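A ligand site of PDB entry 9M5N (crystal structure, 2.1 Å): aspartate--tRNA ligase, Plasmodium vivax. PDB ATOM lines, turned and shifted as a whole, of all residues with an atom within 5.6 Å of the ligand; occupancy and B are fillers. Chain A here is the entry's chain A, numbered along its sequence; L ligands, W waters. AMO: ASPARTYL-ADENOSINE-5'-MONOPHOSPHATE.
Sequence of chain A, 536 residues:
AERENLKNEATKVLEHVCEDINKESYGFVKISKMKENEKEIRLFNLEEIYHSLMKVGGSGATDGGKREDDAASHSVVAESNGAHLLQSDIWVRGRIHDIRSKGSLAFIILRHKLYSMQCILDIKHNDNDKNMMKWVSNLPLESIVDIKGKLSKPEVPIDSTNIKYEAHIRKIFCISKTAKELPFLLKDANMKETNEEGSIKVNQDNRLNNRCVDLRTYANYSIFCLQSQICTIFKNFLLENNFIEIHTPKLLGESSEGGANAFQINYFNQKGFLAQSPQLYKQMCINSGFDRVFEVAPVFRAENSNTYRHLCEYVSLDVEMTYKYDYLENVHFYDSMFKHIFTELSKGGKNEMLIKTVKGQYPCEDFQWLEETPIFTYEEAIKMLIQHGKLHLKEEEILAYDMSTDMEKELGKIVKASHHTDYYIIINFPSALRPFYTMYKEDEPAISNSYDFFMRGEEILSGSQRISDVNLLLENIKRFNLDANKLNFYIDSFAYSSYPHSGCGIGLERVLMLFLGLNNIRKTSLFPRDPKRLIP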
ATOM      1  N   GLN A 276     -12.212 -30.039 -16.239  1.00  0.00           N
ATOM      2  CA  GLN A 276     -13.519 -30.152 -15.593  1.00  0.00           C
ATOM      3  C   GLN A 276     -14.449 -29.024 -15.991  1.00  0.00           C
ATOM      4  O   GLN A 276     -15.662 -29.102 -15.722  1.00  0.00           O
ATOM      5  CB  GLN A 276     -13.350 -30.150 -14.081  1.00  0.00           C
ATOM      6  CG  GLN A 276     -12.390 -31.201 -13.592  1.00  0.00           C
ATOM      7  CD  GLN A 276     -12.127 -31.087 -12.118  1.00  0.00           C
ATOM      8  OE1 GLN A 276     -12.932 -31.540 -11.305  1.00  0.00           O
ATOM      9  NE2 GLN A 276     -11.013 -30.485 -11.752  1.00  0.00           N
ATOM     10  N   SER A 277     -13.914 -28.001 -16.632  1.00  0.00           N
ATOM     11  CA  SER A 277     -14.581 -26.743 -16.894  1.00  0.00           C
ATOM     12  C   SER A 277     -13.673 -25.877 -17.762  1.00  0.00           C
ATOM     13  O   SER A 277     -12.436 -25.942 -17.610  1.00  0.00           O
ATOM     14  CB  SER A 277     -14.902 -26.021 -15.587  1.00  0.00           C
ATOM     15  OG  SER A 277     -15.342 -24.714 -15.878  1.00  0.00           O
ATOM     16  N   GLN A 279     -13.519 -22.790 -17.370  1.00  0.00           N
ATOM     17  CA  GLN A 279     -13.487 -21.602 -16.511  1.00  0.00           C
ATOM     18  C   GLN A 279     -12.315 -20.654 -16.784  1.00  0.00           C
ATOM     19  O   GLN A 279     -12.509 -19.471 -17.111  1.00  0.00           O
ATOM     20  CB  GLN A 279     -13.452 -22.041 -15.044  1.00  0.00           C
ATOM     21  CG  GLN A 279     -13.457 -20.913 -14.035  1.00  0.00           C
ATOM     22  CD  GLN A 279     -14.743 -20.095 -14.095  1.00  0.00           C
ATOM     23  OE1 GLN A 279     -15.825 -20.661 -14.190  1.00  0.00           O
ATOM     24  NE2 GLN A 279     -14.628 -18.766 -14.077  1.00  0.00           N
ATOM     25  N   LYS A 282     -12.160 -19.162 -20.448  1.00  0.00           N
ATOM     26  CA  LYS A 282     -13.175 -18.175 -20.810  1.00  0.00           C
ATOM     27  C   LYS A 282     -12.935 -16.856 -20.088  1.00  0.00           C
ATOM     28  O   LYS A 282     -13.070 -15.773 -20.682  1.00  0.00           O
ATOM     29  CB  LYS A 282     -14.595 -18.715 -20.561  1.00  0.00           C
ATOM     30  CG  LYS A 282     -14.986 -18.958 -19.108  1.00  0.00           C
ATOM     31  CD  LYS A 282     -16.417 -19.519 -19.044  1.00  0.00           C
ATOM     32  CE  LYS A 282     -16.795 -19.991 -17.633  1.00  0.00           C
ATOM     33  NZ  LYS A 282     -18.275 -20.156 -17.492  1.00  0.00           N
ATOM     34  N   ARG A 301     -15.379 -35.131 -15.393  1.00  0.00           N
ATOM     35  CA  ARG A 301     -15.436 -35.090 -13.938  1.00  0.00           C
ATOM     36  C   ARG A 301     -15.131 -36.478 -13.409  1.00  0.00           C
ATOM     37  O   ARG A 301     -15.837 -37.436 -13.737  1.00  0.00           O
ATOM     38  CB  ARG A 301     -16.821 -34.634 -13.440  1.00  0.00           C
ATOM     39  CG  ARG A 301     -17.334 -33.341 -14.038  1.00  0.00           C
ATOM     40  CD  ARG A 301     -16.760 -32.148 -13.278  1.00  0.00           C
ATOM     41  NE  ARG A 301     -17.082 -30.842 -13.868  1.00  0.00           N
ATOM     42  CZ  ARG A 301     -17.846 -29.920 -13.289  1.00  0.00           C
ATOM     43  NH1 ARG A 301     -18.502 -30.169 -12.156  1.00  0.00           N
ATOM     44  NH2 ARG A 301     -17.937 -28.716 -13.840  1.00  0.00           N
ATOM     45  N   ARG A 309     -28.314 -38.132 -11.202  1.00  0.00           N
ATOM     46  CA  ARG A 309     -28.095 -36.876 -11.918  1.00  0.00           C
ATOM     47  C   ARG A 309     -26.663 -36.425 -12.159  1.00  0.00           C
ATOM     48  O   ARG A 309     -26.432 -35.290 -12.502  1.00  0.00           O
ATOM     49  CB  ARG A 309     -28.842 -35.759 -11.210  1.00  0.00           C
ATOM     50  CG  ARG A 309     -28.267 -35.364  -9.871  1.00  0.00           C
ATOM     51  CD  ARG A 309     -29.032 -34.245  -9.201  1.00  0.00           C
ATOM     52  NE  ARG A 309     -28.161 -33.243  -8.598  1.00  0.00           N
ATOM     53  CZ  ARG A 309     -28.583 -32.077  -8.147  1.00  0.00           C
ATOM     54  NH1 ARG A 309     -29.851 -31.778  -8.216  1.00  0.00           N
ATOM     55  NH2 ARG A 309     -27.737 -31.212  -7.625  1.00  0.00           N
ATOM     56  N   HIS A 310     -25.721 -37.329 -12.004  1.00  0.00           N
ATOM     57  CA  HIS A 310     -24.295 -37.049 -12.111  1.00  0.00           C
ATOM     58  C   HIS A 310     -23.695 -37.951 -13.190  1.00  0.00           C
ATOM     59  O   HIS A 310     -23.888 -39.164 -13.155  1.00  0.00           O
ATOM     60  CB  HIS A 310     -23.595 -37.306 -10.765  1.00  0.00           C
ATOM     61  CG  HIS A 310     -22.110 -37.059 -10.782  1.00  0.00           C
ATOM     62  ND1 HIS A 310     -21.530 -35.962 -10.179  1.00  0.00           N
ATOM     63  CD2 HIS A 310     -21.092 -37.788 -11.323  1.00  0.00           C
ATOM     64  CE1 HIS A 310     -20.216 -36.023 -10.344  1.00  0.00           C
ATOM     65  NE2 HIS A 310     -19.929 -37.113 -11.029  1.00  0.00           N
ATOM     66  N   LEU A 311     -22.940 -37.348 -14.125  1.00  0.00           N
ATOM     67  CA  LEU A 311     -22.175 -38.076 -15.130  1.00  0.00           C
ATOM     68  C   LEU A 311     -20.688 -37.753 -14.993  1.00  0.00           C
ATOM     69  O   LEU A 311     -20.310 -36.695 -14.490  1.00  0.00           O
ATOM     70  CB  LEU A 311     -22.628 -37.705 -16.548  1.00  0.00           C
ATOM     71  CG  LEU A 311     -24.096 -37.876 -16.880  1.00  0.00           C
ATOM     72  CD1 LEU A 311     -24.474 -37.068 -18.137  1.00  0.00           C
ATOM     73  CD2 LEU A 311     -24.455 -39.349 -17.006  1.00  0.00           C
ATOM     74  N   CYS A 312     -19.838 -38.659 -15.501  1.00  0.00           N
ATOM     75  CA  CYS A 312     -18.408 -38.391 -15.555  1.00  0.00           C
ATOM     76  C   CYS A 312     -17.989 -37.548 -16.762  1.00  0.00           C
ATOM     77  O   CYS A 312     -16.909 -36.955 -16.750  1.00  0.00           O
ATOM     78  CB  CYS A 312     -17.615 -39.705 -15.559  1.00  0.00           C
ATOM     79  SG  CYS A 312     -17.885 -40.695 -14.063  1.00  0.00           S
ATOM     80  N   TYR A 314     -19.935 -34.678 -19.495  1.00  0.00           N
ATOM     81  CA  TYR A 314     -21.193 -34.074 -19.943  1.00  0.00           C
ATOM     82  C   TYR A 314     -20.900 -32.870 -20.816  1.00  0.00           C
ATOM     83  O   TYR A 314     -19.741 -32.472 -20.974  1.00  0.00           O
ATOM     84  CB  TYR A 314     -22.116 -33.723 -18.765  1.00  0.00           C
ATOM     85  CG  TYR A 314     -21.673 -32.548 -17.878  1.00  0.00           C
ATOM     86  CD1 TYR A 314     -22.184 -31.268 -18.065  1.00  0.00           C
ATOM     87  CD2 TYR A 314     -20.772 -32.752 -16.845  1.00  0.00           C
ATOM     88  CE1 TYR A 314     -21.799 -30.208 -17.238  1.00  0.00           C
ATOM     89  CE2 TYR A 314     -20.385 -31.711 -16.015  1.00  0.00           C
ATOM     90  CZ  TYR A 314     -20.895 -30.444 -16.214  1.00  0.00           C
ATOM     91  OH  TYR A 314     -20.464 -29.402 -15.394  1.00  0.00           O
ATOM     92  N   SER A 316     -21.089 -29.047 -21.270  1.00  0.00           N
ATOM     93  CA  SER A 316     -21.236 -27.790 -20.541  1.00  0.00           C
ATOM     94  C   SER A 316     -21.539 -26.670 -21.530  1.00  0.00           C
ATOM     95  O   SER A 316     -20.894 -26.571 -22.583  1.00  0.00           O
ATOM     96  CB  SER A 316     -19.967 -27.486 -19.753  1.00  0.00           C
ATOM     97  OG  SER A 316     -20.180 -26.407 -18.851  1.00  0.00           O
ATOM     98  N   ASP A 318     -21.294 -22.788 -21.463  1.00  0.00           N
ATOM     99  CA  ASP A 318     -20.587 -21.814 -20.663  1.00  0.00           C
ATOM    100  C   ASP A 318     -20.770 -20.441 -21.264  1.00  0.00           C
ATOM    101  O   ASP A 318     -20.783 -20.287 -22.490  1.00  0.00           O
ATOM    102  CB  ASP A 318     -19.106 -22.146 -20.553  1.00  0.00           C
ATOM    103  CG  ASP A 318     -18.846 -23.211 -19.526  1.00  0.00           C
ATOM    104  OD1 ASP A 318     -18.854 -24.419 -19.898  1.00  0.00           O
ATOM    105  OD2 ASP A 318     -18.647 -22.844 -18.342  1.00  0.00           O
ATOM    106  N   VAL A 319     -20.959 -19.467 -20.385  1.00  0.00           N
ATOM    107  CA  VAL A 319     -21.093 -18.073 -20.754  1.00  0.00           C
ATOM    108  C   VAL A 319     -20.136 -17.287 -19.886  1.00  0.00           C
ATOM    109  O   VAL A 319     -19.951 -17.611 -18.703  1.00  0.00           O
ATOM    110  CB  VAL A 319     -22.534 -17.551 -20.581  1.00  0.00           C
ATOM    111  CG1 VAL A 319     -22.686 -16.173 -21.223  1.00  0.00           C
ATOM    112  CG2 VAL A 319     -23.553 -18.516 -21.147  1.00  0.00           C
ATOM    113  N   GLU A 320     -19.514 -16.250 -20.471  1.00  0.00           N
ATOM    114  CA  GLU A 320     -18.694 -15.315 -19.704  1.00  0.00           C
ATOM    115  C   GLU A 320     -18.798 -13.952 -20.396  1.00  0.00           C
ATOM    116  O   GLU A 320     -18.733 -13.886 -21.630  1.00  0.00           O
ATOM    117  CB  GLU A 320     -17.239 -15.790 -19.596  1.00  0.00           C
ATOM    118  CG  GLU A 320     -16.436 -15.169 -18.443  1.00  0.00           C
ATOM    119  CD  GLU A 320     -16.707 -15.870 -17.101  1.00  0.00           C
ATOM    120  OE1 GLU A 320     -17.296 -16.977 -17.085  1.00  0.00           O
ATOM    121  OE2 GLU A 320     -16.303 -15.301 -16.065  1.00  0.00           O
ATOM    122  N   TYR A 437     -12.322 -17.957  -7.465  1.00  0.00           N
ATOM    123  CA  TYR A 437     -12.472 -16.849  -8.395  1.00  0.00           C
ATOM    124  C   TYR A 437     -13.723 -16.025  -8.114  1.00  0.00           C
ATOM    125  O   TYR A 437     -13.951 -15.023  -8.797  1.00  0.00           O
ATOM    126  CB  TYR A 437     -12.503 -17.352  -9.850  1.00  0.00           C
ATOM    127  CG  TYR A 437     -13.390 -18.560 -10.092  1.00  0.00           C
ATOM    128  CD1 TYR A 437     -12.830 -19.816 -10.336  1.00  0.00           C
ATOM    129  CD2 TYR A 437     -14.784 -18.462 -10.106  1.00  0.00           C
ATOM    130  CE1 TYR A 437     -13.633 -20.925 -10.563  1.00  0.00           C
ATOM    131  CE2 TYR A 437     -15.586 -19.574 -10.347  1.00  0.00           C
ATOM    132  CZ  TYR A 437     -15.001 -20.803 -10.564  1.00  0.00           C
ATOM    133  OH  TYR A 437     -15.768 -21.920 -10.794  1.00  0.00           O
ATOM    134  N   GLU A 459     -30.437 -27.921  -9.312  1.00  0.00           N
ATOM    135  CA  GLU A 459     -29.475 -26.981  -9.870  1.00  0.00           C
ATOM    136  C   GLU A 459     -29.230 -27.247 -11.343  1.00  0.00           C
ATOM    137  O   GLU A 459     -28.964 -28.392 -11.734  1.00  0.00           O
ATOM    138  CB  GLU A 459     -28.177 -27.062  -9.091  1.00  0.00           C
ATOM    139  CG  GLU A 459     -27.076 -26.167  -9.664  1.00  0.00           C
ATOM    140  CD  GLU A 459     -25.731 -26.431  -9.031  1.00  0.00           C
ATOM    141  OE1 GLU A 459     -25.674 -26.695  -7.805  1.00  0.00           O
ATOM    142  OE2 GLU A 459     -24.718 -26.371  -9.776  1.00  0.00           O
ATOM    143  N   ILE A 460     -29.334 -26.203 -12.179  1.00  0.00           N
ATOM    144  CA  ILE A 460     -28.964 -26.300 -13.595  1.00  0.00           C
ATOM    145  C   ILE A 460     -27.788 -25.398 -13.967  1.00  0.00           C
ATOM    146  O   ILE A 460     -27.111 -25.676 -14.980  1.00  0.00           O
ATOM    147  CB  ILE A 460     -30.167 -25.983 -14.516  1.00  0.00           C
ATOM    148  CG1 ILE A 460     -30.904 -24.732 -14.044  1.00  0.00           C
ATOM    149  CG2 ILE A 460     -31.073 -27.173 -14.640  1.00  0.00           C
ATOM    150  CD1 ILE A 460     -31.328 -23.815 -15.179  1.00  0.00           C
ATOM    151  N   LEU A 461     -27.553 -24.328 -13.214  1.00  0.00           N
ATOM    152  CA  LEU A 461     -26.567 -23.309 -13.545  1.00  0.00           C
ATOM    153  C   LEU A 461     -25.853 -22.888 -12.276  1.00  0.00           C
ATOM    154  O   LEU A 461     -26.465 -22.779 -11.202  1.00  0.00           O
ATOM    155  CB  LEU A 461     -27.220 -22.074 -14.198  1.00  0.00           C
ATOM    156  CG  LEU A 461     -26.411 -20.766 -14.376  1.00  0.00           C
ATOM    157  CD1 LEU A 461     -26.957 -19.920 -15.525  1.00  0.00           C
ATOM    158  CD2 LEU A 461     -26.382 -19.919 -13.111  1.00  0.00           C
ATOM    159  N   SER A 462     -24.578 -22.568 -12.396  1.00  0.00           N
ATOM    160  CA  SER A 462     -23.767 -22.080 -11.316  1.00  0.00           C
ATOM    161  C   SER A 462     -22.956 -20.918 -11.887  1.00  0.00           C
ATOM    162  O   SER A 462     -22.505 -21.003 -13.002  1.00  0.00           O
ATOM    163  CB  SER A 462     -22.836 -23.171 -10.874  1.00  0.00           C
ATOM    164  OG  SER A 462     -22.522 -22.995  -9.533  1.00  0.00           O
ATOM    165  N   GLY A 463     -22.755 -19.861 -11.142  1.00  0.00           N
ATOM    166  CA  GLY A 463     -22.021 -18.731 -11.695  1.00  0.00           C
ATOM    167  C   GLY A 463     -21.696 -17.697 -10.639  1.00  0.00           C
ATOM    168  O   GLY A 463     -22.123 -17.797  -9.479  1.00  0.00           O
ATOM    169  N   SER A 464     -20.965 -16.670 -11.075  1.00  0.00           N
ATOM    170  CA  SER A 464     -20.639 -15.586 -10.150  1.00  0.00           C
ATOM    171  C   SER A 464     -19.984 -14.421 -10.895  1.00  0.00           C
ATOM    172  O   SER A 464     -19.486 -14.566 -12.025  1.00  0.00           O
ATOM    173  CB  SER A 464     -19.715 -16.037  -9.018  1.00  0.00           C
ATOM    174  OG  SER A 464     -18.359 -16.096  -9.431  1.00  0.00           O
ATOM    175  N   ARG A 466     -16.776 -12.352 -11.067  1.00  0.00           N
ATOM    176  CA  ARG A 466     -15.413 -12.820 -10.882  1.00  0.00           C
ATOM    177  C   ARG A 466     -14.561 -11.780 -10.165  1.00  0.00           C
ATOM    178  O   ARG A 466     -14.831 -10.583 -10.193  1.00  0.00           O
ATOM    179  CB  ARG A 466     -14.775 -13.163 -12.219  1.00  0.00           C
ATOM    180  CG  ARG A 466     -15.684 -13.965 -13.138  1.00  0.00           C
ATOM    181  CD  ARG A 466     -16.164 -15.280 -12.560  1.00  0.00           C
ATOM    182  NE  ARG A 466     -16.717 -16.088 -13.645  1.00  0.00           N
ATOM    183  CZ  ARG A 466     -17.580 -17.092 -13.513  1.00  0.00           C
ATOM    184  NH1 ARG A 466     -18.039 -17.472 -12.318  1.00  0.00           N
ATOM    185  NH2 ARG A 466     -18.003 -17.730 -14.597  1.00  0.00           N
ATOM    186  N   GLY A 503     -19.762 -14.841 -15.043  1.00  0.00           N
ATOM    187  CA  GLY A 503     -20.103 -15.896 -15.974  1.00  0.00           C
ATOM    188  C   GLY A 503     -20.931 -16.960 -15.291  1.00  0.00           C
ATOM    189  O   GLY A 503     -21.292 -16.828 -14.102  1.00  0.00           O
ATOM    190  N   CYS A 504     -21.222 -18.007 -16.067  1.00  0.00           N
ATOM    191  CA  CYS A 504     -21.970 -19.158 -15.578  1.00  0.00           C
ATOM    192  C   CYS A 504     -21.673 -20.413 -16.408  1.00  0.00           C
ATOM    193  O   CYS A 504     -21.264 -20.345 -17.573  1.00  0.00           O
ATOM    194  CB  CYS A 504     -23.469 -18.884 -15.594  1.00  0.00           C
ATOM    195  SG  CYS A 504     -24.131 -18.520 -17.233  1.00  0.00           S
ATOM    196  N   GLY A 505     -21.873 -21.557 -15.759  1.00  0.00           N
ATOM    197  CA  GLY A 505     -21.821 -22.858 -16.412  1.00  0.00           C
ATOM    198  C   GLY A 505     -23.115 -23.619 -16.195  1.00  0.00           C
ATOM    199  O   GLY A 505     -23.709 -23.579 -15.109  1.00  0.00           O
ATOM    200  N   ILE A 506     -23.542 -24.343 -17.244  1.00  0.00           N
ATOM    201  CA  ILE A 506     -24.870 -24.927 -17.354  1.00  0.00           C
ATOM    202  C   ILE A 506     -24.733 -26.373 -17.810  1.00  0.00           C
ATOM    203  O   ILE A 506     -23.989 -26.659 -18.771  1.00  0.00           O
ATOM    204  CB  ILE A 506     -25.745 -24.147 -18.359  1.00  0.00           C
ATOM    205  CG1 ILE A 506     -25.932 -22.686 -17.917  1.00  0.00           C
ATOM    206  CG2 ILE A 506     -27.072 -24.858 -18.628  1.00  0.00           C
ATOM    207  CD1 ILE A 506     -26.264 -21.746 -19.068  1.00  0.00           C
ATOM    208  N   GLY A 507     -25.462 -27.285 -17.162  1.00  0.00           N
ATOM    209  CA  GLY A 507     -25.466 -28.634 -17.719  1.00  0.00           C
ATOM    210  C   GLY A 507     -26.563 -28.849 -18.763  1.00  0.00           C
ATOM    211  O   GLY A 507     -27.752 -28.751 -18.420  1.00  0.00           O
ATOM    212  N   GLU A 509     -27.531 -31.683 -20.418  1.00  0.00           N
ATOM    213  CA  GLU A 509     -28.338 -32.869 -20.122  1.00  0.00           C
ATOM    214  C   GLU A 509     -29.201 -32.638 -18.891  1.00  0.00           C
ATOM    215  O   GLU A 509     -30.337 -33.140 -18.821  1.00  0.00           O
ATOM    216  CB  GLU A 509     -27.442 -34.110 -19.897  1.00  0.00           C
ATOM    217  CG  GLU A 509     -26.454 -34.402 -21.050  1.00  0.00           C
ATOM    218  CD  GLU A 509     -25.159 -33.577 -21.003  1.00  0.00           C
ATOM    219  OE1 GLU A 509     -25.069 -32.575 -20.246  1.00  0.00           O
ATOM    220  OE2 GLU A 509     -24.209 -33.943 -21.724  1.00  0.00           O
ATOM    221  N   ARG A 510     -28.684 -31.927 -17.888  1.00  0.00           N
ATOM    222  CA  ARG A 510     -29.506 -31.693 -16.718  1.00  0.00           C
ATOM    223  C   ARG A 510     -30.679 -30.757 -17.029  1.00  0.00           C
ATOM    224  O   ARG A 510     -31.792 -30.978 -16.549  1.00  0.00           O
ATOM    225  CB  ARG A 510     -28.686 -31.130 -15.554  1.00  0.00           C
ATOM    226  CG  ARG A 510     -29.249 -31.746 -14.275  1.00  0.00           C
ATOM    227  CD  ARG A 510     -28.614 -31.264 -13.045  1.00  0.00           C
ATOM    228  NE  ARG A 510     -27.571 -32.152 -12.581  1.00  0.00           N
ATOM    229  CZ  ARG A 510     -26.697 -31.776 -11.649  1.00  0.00           C
ATOM    230  NH1 ARG A 510     -26.775 -30.565 -11.100  1.00  0.00           N
ATOM    231  NH2 ARG A 510     -25.728 -32.613 -11.280  1.00  0.00           N
ATOM    232  N   ILE A 521     -30.505 -38.722 -15.522  1.00  0.00           N
ATOM    233  CA  ILE A 521     -29.786 -37.958 -16.514  1.00  0.00           C
ATOM    234  C   ILE A 521     -29.248 -38.858 -17.621  1.00  0.00           C
ATOM    235  O   ILE A 521     -28.919 -38.378 -18.715  1.00  0.00           O
ATOM    236  CB  ILE A 521     -28.657 -37.144 -15.849  1.00  0.00           C
ATOM    237  CG1 ILE A 521     -28.102 -36.092 -16.816  1.00  0.00           C
ATOM    238  CG2 ILE A 521     -27.552 -38.079 -15.321  1.00  0.00           C
ATOM    239  CD1 ILE A 521     -27.385 -34.941 -16.115  1.00  0.00           C
HETATM  240  P   AMO L   1     -20.598 -26.713 -11.551  1.00  0.00           P
HETATM  241  O1P AMO L   1     -19.554 -27.693 -11.281  1.00  0.00           O
HETATM  242  O2P AMO L   1     -21.631 -26.382 -10.582  1.00  0.00           O
HETATM  243  O3P AMO L   1     -20.009 -25.290 -11.754  1.00  0.00           O
HETATM  244  O5' AMO L   1     -21.307 -27.025 -12.901  1.00  0.00           O
HETATM  245  C5' AMO L   1     -22.408 -26.234 -13.255  1.00  0.00           C
HETATM  246  C4' AMO L   1     -23.559 -27.011 -13.870  1.00  0.00           C
HETATM  247  O4' AMO L   1     -23.101 -28.111 -14.617  1.00  0.00           O
HETATM  248  C1' AMO L   1     -23.968 -29.210 -14.449  1.00  0.00           C
HETATM  249  N9  AMO L   1     -23.199 -30.307 -13.856  1.00  0.00           N
HETATM  250  C4  AMO L   1     -23.269 -31.558 -14.220  1.00  0.00           C
HETATM  251  N3  AMO L   1     -23.982 -32.233 -15.118  1.00  0.00           N
HETATM  252  C2  AMO L   1     -23.826 -33.544 -15.248  1.00  0.00           C
HETATM  253  N1  AMO L   1     -22.980 -34.271 -14.534  1.00  0.00           N
HETATM  254  C6  AMO L   1     -22.211 -33.719 -13.604  1.00  0.00           C
HETATM  255  N6  AMO L   1     -21.359 -34.435 -12.884  1.00  0.00           N
HETATM  256  C5  AMO L   1     -22.319 -32.281 -13.395  1.00  0.00           C
HETATM  257  N7  AMO L   1     -21.754 -31.397 -12.602  1.00  0.00           N
HETATM  258  C8  AMO L   1     -22.293 -30.208 -12.892  1.00  0.00           C
HETATM  259  C2' AMO L   1     -25.063 -28.758 -13.519  1.00  0.00           C
HETATM  260  C3' AMO L   1     -24.439 -27.610 -12.805  1.00  0.00           C
HETATM  261  O3' AMO L   1     -25.398 -26.654 -12.387  1.00  0.00           O
HETATM  262  N   AMO L   1     -17.278 -23.432 -13.478  1.00  0.00           N
HETATM  263  CA  AMO L   1     -18.498 -23.511 -12.714  1.00  0.00           C
HETATM  264  CB  AMO L   1     -19.577 -22.590 -13.273  1.00  0.00           C
HETATM  265  CG  AMO L   1     -19.132 -21.155 -13.290  1.00  0.00           C
HETATM  266  OD1 AMO L   1     -19.057 -20.519 -12.218  1.00  0.00           O
HETATM  267  OD2 AMO L   1     -18.867 -20.651 -14.401  1.00  0.00           O
HETATM  268  C   AMO L   1     -18.987 -24.926 -12.690  1.00  0.00           C
HETATM  269  O   AMO L   1     -18.564 -25.754 -13.439  1.00  0.00           O
HETATM  270  O2' AMO L   1     -26.095 -28.273 -14.343  1.00  0.00           O
HETATM  271  O   HOH W   1     -19.403 -32.660 -10.737  1.00  0.00           O
HETATM  272  O   HOH W   2     -14.935 -24.429 -11.662  1.00  0.00           O
HETATM  273  O   HOH W   3     -18.009 -24.093 -16.336  1.00  0.00           O
HETATM  274  O   HOH W   4     -25.597 -31.905 -17.563  1.00  0.00           O
HETATM  275  O   HOH W   5     -19.511 -20.528  -9.492  1.00  0.00           O
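O2' of the ligand lies within hydrogen-bond range of O of Ile 460, at 2.9 Å.
O of Leu 311 sits at hydrogen-bond distance from N6 of the ligand, at 3.0 Å.
The side-chain hydroxyl (OH) of Tyr 314 lies within hydrogen-bond range of an oxygen (O4') of the ligand (3.0 Å).
N of the ligand sits at hydrogen-bond distance from OH of Tyr 437.
N1 of the ligand lies within hydrogen-bond range of N of Leu 311 (3.1 Å).
An oxygen (O1P) of the ligand is in salt-bridge range of the guanidinium group (NH1) of Arg 301 (2.8 Å).
N of Leu 461 lies within hydrogen-bond range of O3' of the ligand, at 3.3 Å.
The side-chain amide oxygen of Gln 279 lies close to an oxygen (OD2) of the ligand.
N of Gly 505 lies within hydrogen-bond range of OD2 of the ligand (3.4 Å).
An oxygen (OD2) of the ligand lies within salt-bridge range of the guanidinium group (NH2) of Arg 466 (3.1 Å).
O3' of the ligand is in hydrogen-bond range of OE2 of Glu 459, 2.7 Å away.
The backbone NH (N) of Gly 507 is in hydrogen-bond range of an oxygen (O2') of the ligand, at 3.1 Å.
The side-chain amino group of Lys 282 lies within salt-bridge range of an oxygen (OD2) of the ligand, 3.2 Å away.
A nitrogen (N6) of the ligand sits at hydrogen-bond distance from a ring nitrogen (ND1) of His 310 (3.1 Å).
The side-chain hydroxyl (OG) of Ser 277 lies within hydrogen-bond range of a nitrogen (N) of the ligand (3.3 Å).
The side-chain amide nitrogen (NE2) of Gln 279 sits close to the guanidinium group (NE) of Arg 466 (3.4 Å).
NH2 of Arg 510 sits at hydrogen-bond distance from O of Arg 309 (3.0 Å).
The backbone NH (N) of Cys 504 sits at hydrogen-bond distance from the backbone carbonyl oxygen (O) of Val 319, 3.0 Å away.
The side-chain amino group (NZ) of Lys 282 is in hydrogen-bond range of the backbone carbonyl oxygen (O) of Val 319, at 3.3 Å.
NH1 of Arg 466 lies within hydrogen-bond range of OG of Ser 464, at 3.2 Å.
NE of Arg 466 is in salt-bridge range of OE2 of Glu 320, 2.6 Å away.
The backbone carbonyl oxygen of Ser 462 lies within hydrogen-bond range of the backbone NH of Gly 505, 2.9 Å away.
N of Gln 279 lies within hydrogen-bond range of OG of Ser 277 (3.0 Å).
Merely in contact with the ligand: Ser 462 (3.3 Å), Cys 504 (3.5 Å), Arg 510 (3.5 Å), Gly 463 (3.5 Å), Ile 521 (3.9 Å) and Ile 506 (3.98 Å).
Hydrophobic or aromatic side chains within 4 Å of the ligand: His 310, Leu 311, Tyr 314 and Ile 521.
Along chain A the residues within 4 Å of the ligand span positions 277 to 521.
Water W4 lies within hydrogen-bond range of OE1 of Glu 509 (2.8 Å), N3 of the ligand (2.9 Å) and N of Arg 510 (3.1 Å).
Water W3 lies within hydrogen-bond range of OD2 of Asp 318 (2.4 Å), OG of Ser 277 (2.8 Å) and N of the ligand (3.0 Å).
Water W2 bridges OH of Tyr 437 and N of the ligand.
Water W1 lies within hydrogen-bond range of NH1 of Arg 301 and N7 of the ligand.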
